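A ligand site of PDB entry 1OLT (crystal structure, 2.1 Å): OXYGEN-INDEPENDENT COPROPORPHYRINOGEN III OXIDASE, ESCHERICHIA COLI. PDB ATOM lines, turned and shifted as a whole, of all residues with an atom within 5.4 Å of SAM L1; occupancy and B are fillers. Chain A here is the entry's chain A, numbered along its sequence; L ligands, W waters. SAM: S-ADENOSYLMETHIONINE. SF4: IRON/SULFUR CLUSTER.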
ATOM      1  N   CYS A  62     -18.089  -1.703 -32.371  1.00  0.00           N
ATOM      2  CA  CYS A  62     -16.725  -1.302 -32.665  1.00  0.00           C
ATOM      3  C   CYS A  62     -16.164  -2.136 -33.830  1.00  0.00           C
ATOM      4  O   CYS A  62     -16.547  -3.282 -34.030  1.00  0.00           O
ATOM      5  CB  CYS A  62     -15.841  -1.442 -31.445  1.00  0.00           C
ATOM      6  SG  CYS A  62     -16.401  -0.560 -29.986  1.00  0.00           S
ATOM      7  N   CYS A  66     -10.116  -3.805 -28.859  1.00  0.00           N
ATOM      8  CA  CYS A  66      -9.087  -3.277 -28.016  1.00  0.00           C
ATOM      9  C   CYS A  66      -8.988  -4.217 -26.810  1.00  0.00           C
ATOM     10  O   CYS A  66      -9.994  -4.407 -26.109  1.00  0.00           O
ATOM     11  CB  CYS A  66      -9.461  -1.875 -27.530  1.00  0.00           C
ATOM     12  SG  CYS A  66      -9.704  -0.639 -28.880  1.00  0.00           S
ATOM     13  N   PHE A  68      -7.635  -3.868 -23.814  1.00  0.00           N
ATOM     14  CA  PHE A  68      -7.833  -3.244 -22.488  1.00  0.00           C
ATOM     15  C   PHE A  68      -9.306  -2.976 -22.180  1.00  0.00           C
ATOM     16  O   PHE A  68      -9.662  -2.690 -21.041  1.00  0.00           O
ATOM     17  CB  PHE A  68      -7.047  -1.911 -22.384  1.00  0.00           C
ATOM     18  CG  PHE A  68      -7.497  -0.890 -23.393  1.00  0.00           C
ATOM     19  CD1 PHE A  68      -8.681  -0.206 -23.242  1.00  0.00           C
ATOM     20  CD2 PHE A  68      -6.771  -0.673 -24.520  1.00  0.00           C
ATOM     21  CE1 PHE A  68      -9.130   0.685 -24.212  1.00  0.00           C
ATOM     22  CE2 PHE A  68      -7.220   0.203 -25.516  1.00  0.00           C
ATOM     23  CZ  PHE A  68      -8.417   0.877 -25.347  1.00  0.00           C
ATOM     24  N   CYS A  69     -10.181  -3.043 -23.180  1.00  0.00           N
ATOM     25  CA  CYS A  69     -11.459  -2.383 -23.049  1.00  0.00           C
ATOM     26  C   CYS A  69     -12.475  -3.069 -22.172  1.00  0.00           C
ATOM     27  O   CYS A  69     -12.744  -4.201 -22.358  1.00  0.00           O
ATOM     28  CB  CYS A  69     -12.097  -2.061 -24.443  1.00  0.00           C
ATOM     29  SG  CYS A  69     -13.664  -1.208 -24.326  1.00  0.00           S
ATOM     30  N   GLY A  70     -13.074  -2.283 -21.233  1.00  0.00           N
ATOM     31  CA  GLY A  70     -14.051  -2.728 -20.286  1.00  0.00           C
ATOM     32  C   GLY A  70     -15.435  -2.187 -20.558  1.00  0.00           C
ATOM     33  O   GLY A  70     -16.337  -2.374 -19.767  1.00  0.00           O
ATOM     34  N   CYS A  71     -15.656  -1.540 -21.713  1.00  0.00           N
ATOM     35  CA  CYS A  71     -16.953  -0.879 -22.006  1.00  0.00           C
ATOM     36  C   CYS A  71     -18.023  -1.928 -22.417  1.00  0.00           C
ATOM     37  O   CYS A  71     -17.664  -3.066 -22.754  1.00  0.00           O
ATOM     38  CB  CYS A  71     -16.786   0.163 -23.124  1.00  0.00           C
ATOM     39  SG  CYS A  71     -15.420   1.334 -22.888  1.00  0.00           S
ATOM     40  N   GLY A 112     -20.611   4.696 -26.237  1.00  0.00           N
ATOM     41  CA  GLY A 112     -20.517   3.306 -26.659  1.00  0.00           C
ATOM     42  C   GLY A 112     -19.363   2.565 -26.009  1.00  0.00           C
ATOM     43  O   GLY A 112     -19.065   2.826 -24.815  1.00  0.00           O
ATOM     44  N   GLY A 113     -18.679   1.644 -26.735  1.00  0.00           N
ATOM     45  CA  GLY A 113     -18.820   1.413 -28.119  1.00  0.00           C
ATOM     46  C   GLY A 113     -18.298   2.560 -28.896  1.00  0.00           C
ATOM     47  O   GLY A 113     -17.732   3.508 -28.344  1.00  0.00           O
ATOM     48  N   THR A 114     -18.520   2.525 -30.218  1.00  0.00           N
ATOM     49  CA  THR A 114     -18.028   3.514 -31.101  1.00  0.00           C
ATOM     50  C   THR A 114     -19.157   4.157 -31.891  1.00  0.00           C
ATOM     51  O   THR A 114     -19.621   3.603 -32.907  1.00  0.00           O
ATOM     52  CB  THR A 114     -17.037   2.892 -32.078  1.00  0.00           C
ATOM     53  OG1 THR A 114     -15.916   2.294 -31.439  1.00  0.00           O
ATOM     54  CG2 THR A 114     -16.412   4.001 -32.938  1.00  0.00           C
ATOM     55  N   PRO A 115     -19.656   5.313 -31.437  1.00  0.00           N
ATOM     56  CA  PRO A 115     -20.719   6.000 -32.184  1.00  0.00           C
ATOM     57  C   PRO A 115     -20.434   6.239 -33.652  1.00  0.00           C
ATOM     58  O   PRO A 115     -21.390   6.128 -34.432  1.00  0.00           O
ATOM     59  CB  PRO A 115     -20.889   7.328 -31.428  1.00  0.00           C
ATOM     60  CG  PRO A 115     -20.532   6.945 -29.997  1.00  0.00           C
ATOM     61  CD  PRO A 115     -19.418   5.950 -30.145  1.00  0.00           C
ATOM     62  N   GLU A 145     -18.668  10.491 -29.084  1.00  0.00           N
ATOM     63  CA  GLU A 145     -17.350   9.886 -28.994  1.00  0.00           C
ATOM     64  C   GLU A 145     -16.895   9.287 -30.290  1.00  0.00           C
ATOM     65  O   GLU A 145     -17.688   8.708 -31.036  1.00  0.00           O
ATOM     66  CB  GLU A 145     -17.362   8.845 -27.890  1.00  0.00           C
ATOM     67  CG  GLU A 145     -17.940   9.400 -26.580  1.00  0.00           C
ATOM     68  CD  GLU A 145     -17.797   8.519 -25.395  1.00  0.00           C
ATOM     69  OE1 GLU A 145     -16.634   8.023 -25.182  1.00  0.00           O
ATOM     70  OE2 GLU A 145     -18.827   8.336 -24.653  1.00  0.00           O
ATOM     71  N   VAL A 146     -15.590   9.391 -30.554  1.00  0.00           N
ATOM     72  CA  VAL A 146     -15.045   9.133 -31.893  1.00  0.00           C
ATOM     73  C   VAL A 146     -13.812   8.278 -31.742  1.00  0.00           C
ATOM     74  O   VAL A 146     -12.917   8.641 -31.001  1.00  0.00           O
ATOM     75  CB  VAL A 146     -14.641  10.451 -32.606  1.00  0.00           C
ATOM     76  CG1 VAL A 146     -14.041  10.140 -33.973  1.00  0.00           C
ATOM     77  CG2 VAL A 146     -15.830  11.365 -32.779  1.00  0.00           C
ATOM     78  N   ASP A 147     -13.758   7.176 -32.441  1.00  0.00           N
ATOM     79  CA  ASP A 147     -12.529   6.365 -32.567  1.00  0.00           C
ATOM     80  C   ASP A 147     -11.752   6.896 -33.803  1.00  0.00           C
ATOM     81  O   ASP A 147     -12.292   6.918 -34.913  1.00  0.00           O
ATOM     82  CB  ASP A 147     -12.966   4.922 -32.795  1.00  0.00           C
ATOM     83  CG  ASP A 147     -11.822   3.957 -33.086  1.00  0.00           C
ATOM     84  OD1 ASP A 147     -10.649   4.231 -32.733  1.00  0.00           O
ATOM     85  OD2 ASP A 147     -12.061   2.850 -33.631  1.00  0.00           O
ATOM     86  N   PRO A 148     -10.492   7.309 -33.644  1.00  0.00           N
ATOM     87  CA  PRO A 148      -9.771   7.928 -34.768  1.00  0.00           C
ATOM     88  C   PRO A 148      -9.094   6.854 -35.705  1.00  0.00           C
ATOM     89  O   PRO A 148      -7.841   6.939 -36.004  1.00  0.00           O
ATOM     90  CB  PRO A 148      -8.715   8.732 -34.069  1.00  0.00           C
ATOM     91  CG  PRO A 148      -8.352   7.791 -32.853  1.00  0.00           C
ATOM     92  CD  PRO A 148      -9.708   7.294 -32.413  1.00  0.00           C
ATOM     93  N   ARG A 149      -9.856   5.843 -36.059  1.00  0.00           N
ATOM     94  CA  ARG A 149      -9.438   4.766 -36.970  1.00  0.00           C
ATOM     95  C   ARG A 149     -10.618   4.488 -37.873  1.00  0.00           C
ATOM     96  O   ARG A 149     -11.753   4.694 -37.486  1.00  0.00           O
ATOM     97  CB  ARG A 149      -9.120   3.509 -36.207  1.00  0.00           C
ATOM     98  CG  ARG A 149      -7.884   3.598 -35.405  1.00  0.00           C
ATOM     99  CD  ARG A 149      -7.666   2.351 -34.543  1.00  0.00           C
ATOM    100  NE  ARG A 149      -8.670   2.268 -33.467  1.00  0.00           N
ATOM    101  CZ  ARG A 149      -8.965   1.192 -32.777  1.00  0.00           C
ATOM    102  NH1 ARG A 149      -8.292   0.053 -32.978  1.00  0.00           N
ATOM    103  NH2 ARG A 149      -9.889   1.248 -31.814  1.00  0.00           N
ATOM    104  N   MET A 169     -12.454  11.902 -28.171  1.00  0.00           N
ATOM    105  CA  MET A 169     -11.732  11.010 -29.016  1.00  0.00           C
ATOM    106  C   MET A 169     -10.825  10.148 -28.170  1.00  0.00           C
ATOM    107  O   MET A 169     -10.053  10.647 -27.366  1.00  0.00           O
ATOM    108  CB  MET A 169     -10.923  11.827 -30.023  1.00  0.00           C
ATOM    109  CG  MET A 169      -9.975  11.071 -30.924  1.00  0.00           C
ATOM    110  SD  MET A 169      -8.988  12.172 -32.035  1.00  0.00           S
ATOM    111  CE  MET A 169     -10.350  13.168 -32.678  1.00  0.00           C
ATOM    112  N   GLY A 170     -10.932   8.848 -28.354  1.00  0.00           N
ATOM    113  CA  GLY A 170     -10.050   7.924 -27.690  1.00  0.00           C
ATOM    114  C   GLY A 170      -8.654   7.950 -28.301  1.00  0.00           C
ATOM    115  O   GLY A 170      -8.517   7.822 -29.505  1.00  0.00           O
ATOM    116  N   VAL A 171      -7.641   8.060 -27.476  1.00  0.00           N
ATOM    117  CA  VAL A 171      -6.242   7.914 -27.932  1.00  0.00           C
ATOM    118  C   VAL A 171      -5.523   6.765 -27.198  1.00  0.00           C
ATOM    119  O   VAL A 171      -4.881   5.903 -27.796  1.00  0.00           O
ATOM    120  CB  VAL A 171      -5.485   9.272 -27.797  1.00  0.00           C
ATOM    121  CG1 VAL A 171      -3.991   9.133 -27.971  1.00  0.00           C
ATOM    122  CG2 VAL A 171      -6.085  10.328 -28.790  1.00  0.00           C
ATOM    123  N   GLN A 172      -5.713   6.725 -25.877  1.00  0.00           N
ATOM    124  CA  GLN A 172      -5.172   5.750 -24.975  1.00  0.00           C
ATOM    125  C   GLN A 172      -3.680   5.916 -24.735  1.00  0.00           C
ATOM    126  O   GLN A 172      -3.274   6.186 -23.582  1.00  0.00           O
ATOM    127  CB  GLN A 172      -5.555   4.290 -25.354  1.00  0.00           C
ATOM    128  CG  GLN A 172      -6.900   4.157 -26.073  1.00  0.00           C
ATOM    129  CD  GLN A 172      -8.078   4.776 -25.391  1.00  0.00           C
ATOM    130  OE1 GLN A 172      -9.168   4.734 -25.921  1.00  0.00           O
ATOM    131  NE2 GLN A 172      -7.898   5.310 -24.224  1.00  0.00           N
ATOM    132  N   ARG A 184      -4.419  -1.710 -30.578  1.00  0.00           N
ATOM    133  CA  ARG A 184      -4.957  -0.415 -30.914  1.00  0.00           C
ATOM    134  C   ARG A 184      -3.928   0.427 -31.718  1.00  0.00           C
ATOM    135  O   ARG A 184      -3.672   1.588 -31.445  1.00  0.00           O
ATOM    136  CB  ARG A 184      -5.436   0.386 -29.709  1.00  0.00           C
ATOM    137  CG  ARG A 184      -6.476   1.500 -30.168  1.00  0.00           C
ATOM    138  CD  ARG A 184      -6.691   2.400 -29.170  1.00  0.00           C
ATOM    139  NE  ARG A 184      -7.454   3.549 -29.571  1.00  0.00           N
ATOM    140  CZ  ARG A 184      -8.736   3.773 -29.320  1.00  0.00           C
ATOM    141  NH1 ARG A 184      -9.520   2.860 -28.742  1.00  0.00           N
ATOM    142  NH2 ARG A 184      -9.230   4.967 -29.669  1.00  0.00           N
ATOM    143  N   ASP A 209      -9.221  10.848 -24.467  1.00  0.00           N
ATOM    144  CA  ASP A 209      -8.993   9.828 -23.468  1.00  0.00           C
ATOM    145  C   ASP A 209      -7.595   9.223 -23.574  1.00  0.00           C
ATOM    146  O   ASP A 209      -7.114   8.909 -24.686  1.00  0.00           O
ATOM    147  CB  ASP A 209      -9.961   8.658 -23.593  1.00  0.00           C
ATOM    148  CG  ASP A 209     -11.403   9.039 -23.487  1.00  0.00           C
ATOM    149  OD1 ASP A 209     -11.776  10.051 -22.838  1.00  0.00           O
ATOM    150  OD2 ASP A 209     -12.293   8.288 -23.998  1.00  0.00           O
ATOM    151  N   LEU A 210      -6.917   9.143 -22.421  1.00  0.00           N
ATOM    152  CA  LEU A 210      -5.695   8.456 -22.249  1.00  0.00           C
ATOM    153  C   LEU A 210      -5.892   7.419 -21.135  1.00  0.00           C
ATOM    154  O   LEU A 210      -6.755   7.583 -20.268  1.00  0.00           O
ATOM    155  CB  LEU A 210      -4.541   9.381 -21.896  1.00  0.00           C
ATOM    156  CG  LEU A 210      -4.210  10.483 -22.899  1.00  0.00           C
ATOM    157  CD1 LEU A 210      -3.166  11.495 -22.295  1.00  0.00           C
ATOM    158  CD2 LEU A 210      -3.681   9.827 -24.117  1.00  0.00           C
ATOM    159  N   ILE A 211      -5.099   6.346 -21.190  1.00  0.00           N
ATOM    160  CA  ILE A 211      -5.059   5.353 -20.102  1.00  0.00           C
ATOM    161  C   ILE A 211      -3.646   5.134 -19.622  1.00  0.00           C
ATOM    162  O   ILE A 211      -2.712   4.936 -20.436  1.00  0.00           O
ATOM    163  CB  ILE A 211      -5.673   4.014 -20.513  1.00  0.00           C
ATOM    164  CG1 ILE A 211      -7.066   4.179 -21.101  1.00  0.00           C
ATOM    165  CG2 ILE A 211      -5.647   3.036 -19.365  1.00  0.00           C
ATOM    166  CD1 ILE A 211      -7.592   2.846 -21.757  1.00  0.00           C
ATOM    167  N   PHE A 240      -7.473   7.853 -17.487  1.00  0.00           N
ATOM    168  CA  PHE A 240      -8.027   6.769 -16.676  1.00  0.00           C
ATOM    169  C   PHE A 240      -6.972   5.839 -16.217  1.00  0.00           C
ATOM    170  O   PHE A 240      -6.009   5.520 -16.940  1.00  0.00           O
ATOM    171  CB  PHE A 240      -9.044   5.984 -17.511  1.00  0.00           C
ATOM    172  CG  PHE A 240     -10.158   6.835 -18.051  1.00  0.00           C
ATOM    173  CD1 PHE A 240     -11.049   7.447 -17.173  1.00  0.00           C
ATOM    174  CD2 PHE A 240     -10.323   7.035 -19.391  1.00  0.00           C
ATOM    175  CE1 PHE A 240     -12.121   8.234 -17.643  1.00  0.00           C
ATOM    176  CE2 PHE A 240     -11.412   7.819 -19.894  1.00  0.00           C
ATOM    177  CZ  PHE A 240     -12.284   8.432 -19.005  1.00  0.00           C
ATOM    178  N   ASN A 241      -7.116   5.393 -15.011  1.00  0.00           N
ATOM    179  CA  ASN A 241      -6.288   4.328 -14.474  1.00  0.00           C
ATOM    180  C   ASN A 241      -6.790   2.982 -15.100  1.00  0.00           C
ATOM    181  O   ASN A 241      -7.983   2.691 -15.076  1.00  0.00           O
ATOM    182  CB  ASN A 241      -6.452   4.269 -12.947  1.00  0.00           C
ATOM    183  CG  ASN A 241      -5.638   3.124 -12.330  1.00  0.00           C
ATOM    184  OD1 ASN A 241      -4.485   2.941 -12.649  1.00  0.00           O
ATOM    185  ND2 ASN A 241      -6.242   2.373 -11.512  1.00  0.00           N
ATOM    186  N   TYR A 242      -5.888   2.172 -15.638  1.00  0.00           N
ATOM    187  CA  TYR A 242      -6.347   0.925 -16.297  1.00  0.00           C
ATOM    188  C   TYR A 242      -6.993   0.004 -15.279  1.00  0.00           C
ATOM    189  O   TYR A 242      -6.377  -0.405 -14.341  1.00  0.00           O
ATOM    190  CB  TYR A 242      -5.178   0.238 -17.021  1.00  0.00           C
ATOM    191  CG  TYR A 242      -5.516  -1.093 -17.611  1.00  0.00           C
ATOM    192  CD1 TYR A 242      -6.660  -1.267 -18.376  1.00  0.00           C
ATOM    193  CD2 TYR A 242      -4.730  -2.198 -17.350  1.00  0.00           C
ATOM    194  CE1 TYR A 242      -6.967  -2.520 -18.919  1.00  0.00           C
ATOM    195  CE2 TYR A 242      -5.052  -3.432 -17.822  1.00  0.00           C
ATOM    196  CZ  TYR A 242      -6.165  -3.582 -18.636  1.00  0.00           C
ATOM    197  OH  TYR A 242      -6.475  -4.839 -19.061  1.00  0.00           O
ATOM    198  N   ALA A 243      -8.236  -0.370 -15.529  1.00  0.00           N
ATOM    199  CA  ALA A 243      -8.901  -1.373 -14.683  1.00  0.00           C
ATOM    200  C   ALA A 243      -8.808  -2.742 -15.358  1.00  0.00           C
ATOM    201  O   ALA A 243      -9.394  -2.956 -16.450  1.00  0.00           O
ATOM    202  CB  ALA A 243     -10.362  -1.012 -14.519  1.00  0.00           C
ATOM    203  N   HIS A 244      -8.090  -3.635 -14.733  1.00  0.00           N
ATOM    204  CA  HIS A 244      -7.718  -4.936 -15.312  1.00  0.00           C
ATOM    205  C   HIS A 244      -8.507  -6.005 -14.576  1.00  0.00           C
ATOM    206  O   HIS A 244      -8.323  -6.187 -13.384  1.00  0.00           O
ATOM    207  CB  HIS A 244      -6.231  -5.185 -15.102  1.00  0.00           C
ATOM    208  CG  HIS A 244      -5.713  -6.419 -15.788  1.00  0.00           C
ATOM    209  ND1 HIS A 244      -5.753  -6.596 -17.157  1.00  0.00           N
ATOM    210  CD2 HIS A 244      -5.092  -7.513 -15.290  1.00  0.00           C
ATOM    211  CE1 HIS A 244      -5.208  -7.759 -17.458  1.00  0.00           C
ATOM    212  NE2 HIS A 244      -4.808  -8.342 -16.340  1.00  0.00           N
ATOM    213  N   GLN A 252      -8.984  -8.804 -22.202  1.00  0.00           N
ATOM    214  CA  GLN A 252      -7.841  -8.471 -21.342  1.00  0.00           C
ATOM    215  C   GLN A 252      -6.976  -9.676 -21.037  1.00  0.00           C
ATOM    216  O   GLN A 252      -5.813  -9.520 -20.605  1.00  0.00           O
ATOM    217  CB  GLN A 252      -8.308  -7.784 -20.061  1.00  0.00           C
ATOM    218  CG  GLN A 252      -9.117  -6.504 -20.272  1.00  0.00           C
ATOM    219  CD  GLN A 252      -9.590  -5.957 -18.889  1.00  0.00           C
ATOM    220  OE1 GLN A 252      -9.551  -6.700 -17.942  1.00  0.00           O
ATOM    221  NE2 GLN A 252      -9.917  -4.666 -18.788  1.00  0.00           N
HETATM  222  N   SAM L   1     -14.913   3.763 -28.946  1.00  0.00           N
HETATM  223  CA  SAM L   1     -14.176   5.021 -28.995  1.00  0.00           C
HETATM  224  C   SAM L   1     -12.655   4.867 -28.851  1.00  0.00           C
HETATM  225  O   SAM L   1     -12.197   3.792 -28.329  1.00  0.00           O
HETATM  226  OXT SAM L   1     -12.006   5.775 -29.311  1.00  0.00           O
HETATM  227  CB  SAM L   1     -14.712   5.881 -27.835  1.00  0.00           C
HETATM  228  CG  SAM L   1     -14.135   5.772 -26.446  1.00  0.00           C
HETATM  229  SD  SAM L   1     -14.507   4.286 -25.559  1.00  0.00           S
HETATM  230  CE  SAM L   1     -16.298   4.155 -25.597  1.00  0.00           C
HETATM  231  C5' SAM L   1     -14.523   4.915 -23.789  1.00  0.00           C
HETATM  232  C4' SAM L   1     -13.171   5.018 -22.996  1.00  0.00           C
HETATM  233  O4' SAM L   1     -13.064   4.117 -21.903  1.00  0.00           O
HETATM  234  C3' SAM L   1     -11.957   4.673 -23.822  1.00  0.00           C
HETATM  235  O3' SAM L   1     -11.589   5.674 -24.779  1.00  0.00           O
HETATM  236  C2' SAM L   1     -10.888   4.344 -22.772  1.00  0.00           C
HETATM  237  O2' SAM L   1     -10.097   5.484 -22.468  1.00  0.00           O
HETATM  238  C1' SAM L   1     -11.711   3.990 -21.556  1.00  0.00           C
HETATM  239  N9  SAM L   1     -11.506   2.629 -21.088  1.00  0.00           N
HETATM  240  C8  SAM L   1     -12.027   1.511 -21.693  1.00  0.00           C
HETATM  241  N7  SAM L   1     -11.679   0.437 -20.987  1.00  0.00           N
HETATM  242  C5  SAM L   1     -10.948   0.864 -19.913  1.00  0.00           C
HETATM  243  C6  SAM L   1     -10.333   0.196 -18.852  1.00  0.00           C
HETATM  244  N6  SAM L   1     -10.388  -1.132 -18.688  1.00  0.00           N
HETATM  245  N1  SAM L   1      -9.659   0.942 -17.923  1.00  0.00           N
HETATM  246  C2  SAM L   1      -9.585   2.332 -18.053  1.00  0.00           C
HETATM  247  N3  SAM L   1     -10.177   2.984 -19.071  1.00  0.00           N
HETATM  248  C4  SAM L   1     -10.839   2.249 -19.994  1.00  0.00           C
HETATM  249 FE1  SF4 L   2     -14.434  -0.117 -28.862  1.00  0.00          FE
HETATM  250 FE2  SF4 L   2     -13.498  -0.068 -26.371  1.00  0.00          FE
HETATM  251 FE3  SF4 L   2     -13.425   1.960 -27.929  1.00  0.00          FE
HETATM  252 FE4  SF4 L   2     -12.013   0.099 -28.314  1.00  0.00          FE
HETATM  253  S1  SF4 L   2     -11.806   1.410 -26.448  1.00  0.00           S
HETATM  254  S2  SF4 L   2     -12.984   1.144 -30.009  1.00  0.00           S
HETATM  255  S3  SF4 L   2     -13.212  -1.599 -27.955  1.00  0.00           S
HETATM  256  S4  SF4 L   2     -15.176   0.991 -27.105  1.00  0.00           S
HETATM  257  N   SAM L   3     -16.725   3.655 -18.090  1.00  0.00           N
HETATM  258  CA  SAM L   3     -15.304   3.897 -18.433  1.00  0.00           C
HETATM  259  C   SAM L   3     -14.358   3.306 -17.360  1.00  0.00           C
HETATM  260  O   SAM L   3     -13.481   2.463 -17.615  1.00  0.00           O
HETATM  261  OXT SAM L   3     -14.408   3.621 -16.160  1.00  0.00           O
HETATM  262  CB  SAM L   3     -15.056   5.403 -18.653  1.00  0.00           C
HETATM  263  CG  SAM L   3     -15.752   6.034 -19.899  1.00  0.00           C
HETATM  264  SD  SAM L   3     -17.167   7.129 -19.518  1.00  0.00           S
HETATM  265  CE  SAM L   3     -16.405   8.783 -19.584  1.00  0.00           C
HETATM  266  C5' SAM L   3     -18.289   7.251 -20.956  1.00  0.00           C
HETATM  267  C4' SAM L   3     -18.908   5.911 -21.309  1.00  0.00           C
HETATM  268  O4' SAM L   3     -19.776   5.574 -20.229  1.00  0.00           O
HETATM  269  C3' SAM L   3     -19.814   5.926 -22.551  1.00  0.00           C
HETATM  270  O3' SAM L   3     -19.052   5.919 -23.747  1.00  0.00           O
HETATM  271  C2' SAM L   3     -20.666   4.728 -22.259  1.00  0.00           C
HETATM  272  O2' SAM L   3     -19.927   3.548 -22.483  1.00  0.00           O
HETATM  273  C1' SAM L   3     -20.922   4.868 -20.752  1.00  0.00           C
HETATM  274  N9  SAM L   3     -22.101   5.658 -20.453  1.00  0.00           N
HETATM  275  C8  SAM L   3     -22.206   7.013 -20.390  1.00  0.00           C
HETATM  276  N7  SAM L   3     -23.524   7.337 -20.103  1.00  0.00           N
HETATM  277  C5  SAM L   3     -24.214   6.235 -20.005  1.00  0.00           C
HETATM  278  C6  SAM L   3     -25.535   5.988 -19.752  1.00  0.00           C
HETATM  279  N6  SAM L   3     -26.422   6.938 -19.500  1.00  0.00           N
HETATM  280  N1  SAM L   3     -25.924   4.701 -19.746  1.00  0.00           N
HETATM  281  C2  SAM L   3     -25.071   3.695 -19.966  1.00  0.00           C
HETATM  282  N3  SAM L   3     -23.775   3.914 -20.238  1.00  0.00           N
HETATM  283  C4  SAM L   3     -23.360   5.169 -20.248  1.00  0.00           C
HETATM  284  O   HOH W   1     -15.692   7.805 -22.746  1.00  0.00           O
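O of Val 146 sits close to OXT of SAM L1, 3.4 Å away.
Merely in contact with SAM L1: Cys 69 (3.5 Å), Gly 112 (3.2 Å), Glu 145 (3.6 Å), Asp 147 (3.4 Å), Ile 211 (3.6 Å), Phe 240 (3.5 Å), Asn 241 (3.4 Å), Tyr 242 (3.7 Å) and Gln 252 (3.6 Å).
Hydrophobic or aromatic side chains within 4 Å of SAM L1: Phe 68, Ile 211, Phe 240, Tyr 242 and Ala 243.
Within 4 Å of SAM L1: Phe 68, Cys 69, Gly 70, Cys 71, Gly 112, Gly 113, Thr 114, Glu 145, Val 146, Asp 147, Gly 170, Gln 172, Arg 184, Asp 209, Ile 211, Phe 240, Asn 241, Tyr 242, Ala 243 and Gln 252.
The nearest printed residue that does not touch SAM L1 is Pro 148 (4.1 Å).
O of SAM L1 binds FE3 of SF4 L2 (2.2 Å).
OD2 of Asp 209 is in hydrogen-bond range of O3' of SAM L1.
The side-chain amide nitrogen of Gln 172 is in hydrogen-bond range of an oxygen (O2') of SAM L1, at 2.8 Å.
OXT of SAM L1 lies within salt-bridge range of NH2 of Arg 184 (2.9 Å).
The backbone carbonyl oxygen (O) of Gly 113 sits close to a nitrogen (N) of SAM L1 (2.9 Å).
A nitrogen (N6) of SAM L1 lies within hydrogen-bond range of the backbone carbonyl oxygen of Phe 68, at 2.9 Å.
The backbone NH (N) of Ala 243 lies within hydrogen-bond range of a nitrogen (N1) of SAM L1 (3.1 Å).
O of Ala 243 lies within hydrogen-bond range of N6 of SAM L1, 3.1 Å away.
The side-chain hydroxyl (OG1) of Thr 114 lies close to a nitrogen (N) of SAM L1, at 3.1 Å.
The backbone NH of Gly 70 is in hydrogen-bond range of a nitrogen (N7) of SAM L1 (3.1 Å).
The backbone NH (N) of Gly 170 sits close to an oxygen (OXT) of SAM L1 (3.4 Å).
The side-chain sulfur (SG) of Cys 71 sits close to an oxygen (O4') of SAM L1, 3.8 Å away.
NH1 of Arg 184 sits close to S1 of SF4 L2, 3.5 Å away.
The backbone NH (N) of Gly 113 sits close to a sulfur (S4) of SF4 L2, at 3.6 Å.
The side-chain hydroxyl (OG1) of Thr 114 lies close to a sulfur (S2) of SF4 L2 (3.5 Å).
FE2 of SF4 L2 is bound by SG of Cys 69 (2.3 Å).
The side-chain sulfur of Cys 62 binds an iron atom (FE1) of SF4 L2, 2.3 Å away.
NH2 of Arg 149 sits close to S2 of SF4 L2, 3.6 Å away.
SG of Cys 66 binds FE4 of SF4 L2, at 2.5 Å.
The backbone NH of Gly 112 is in hydrogen-bond range of an oxygen (O3') of SAM L3, 3.2 Å away.
The backbone carbonyl oxygen (O) of Gly 112 is in hydrogen-bond range of an oxygen (O2') of SAM L3 (2.6 Å).
The side-chain carboxylate of Glu 145 lies within hydrogen-bond range of an oxygen (O3') of SAM L3.
The backbone carbonyl oxygen of Asp 209 sits at hydrogen-bond distance from the backbone NH of Gln 172, at 2.9 Å.
O of Met 169 lies within hydrogen-bond range of N of Asp 209.
O of Asp 209 is in hydrogen-bond range of N of Val 171 (3.0 Å).
The guanidinium group (NH2) of Arg 184 lies within hydrogen-bond range of the backbone carbonyl oxygen (O) of Gly 170 (2.9 Å).
The side-chain sulfur (SG) of Cys 66 sits close to the guanidinium group (NH1) of Arg 184, 3.5 Å away.
The backbone carbonyl oxygen of Ala 243 lies within hydrogen-bond range of the side-chain amide nitrogen of Gln 252 (2.9 Å).
The side-chain carboxylate (OD1) of Asp 147 is in salt-bridge range of the guanidinium group (NE) of Arg 149, at 2.9 Å.
N of Phe 240 is in hydrogen-bond range of O of Leu 210 (2.9 Å).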
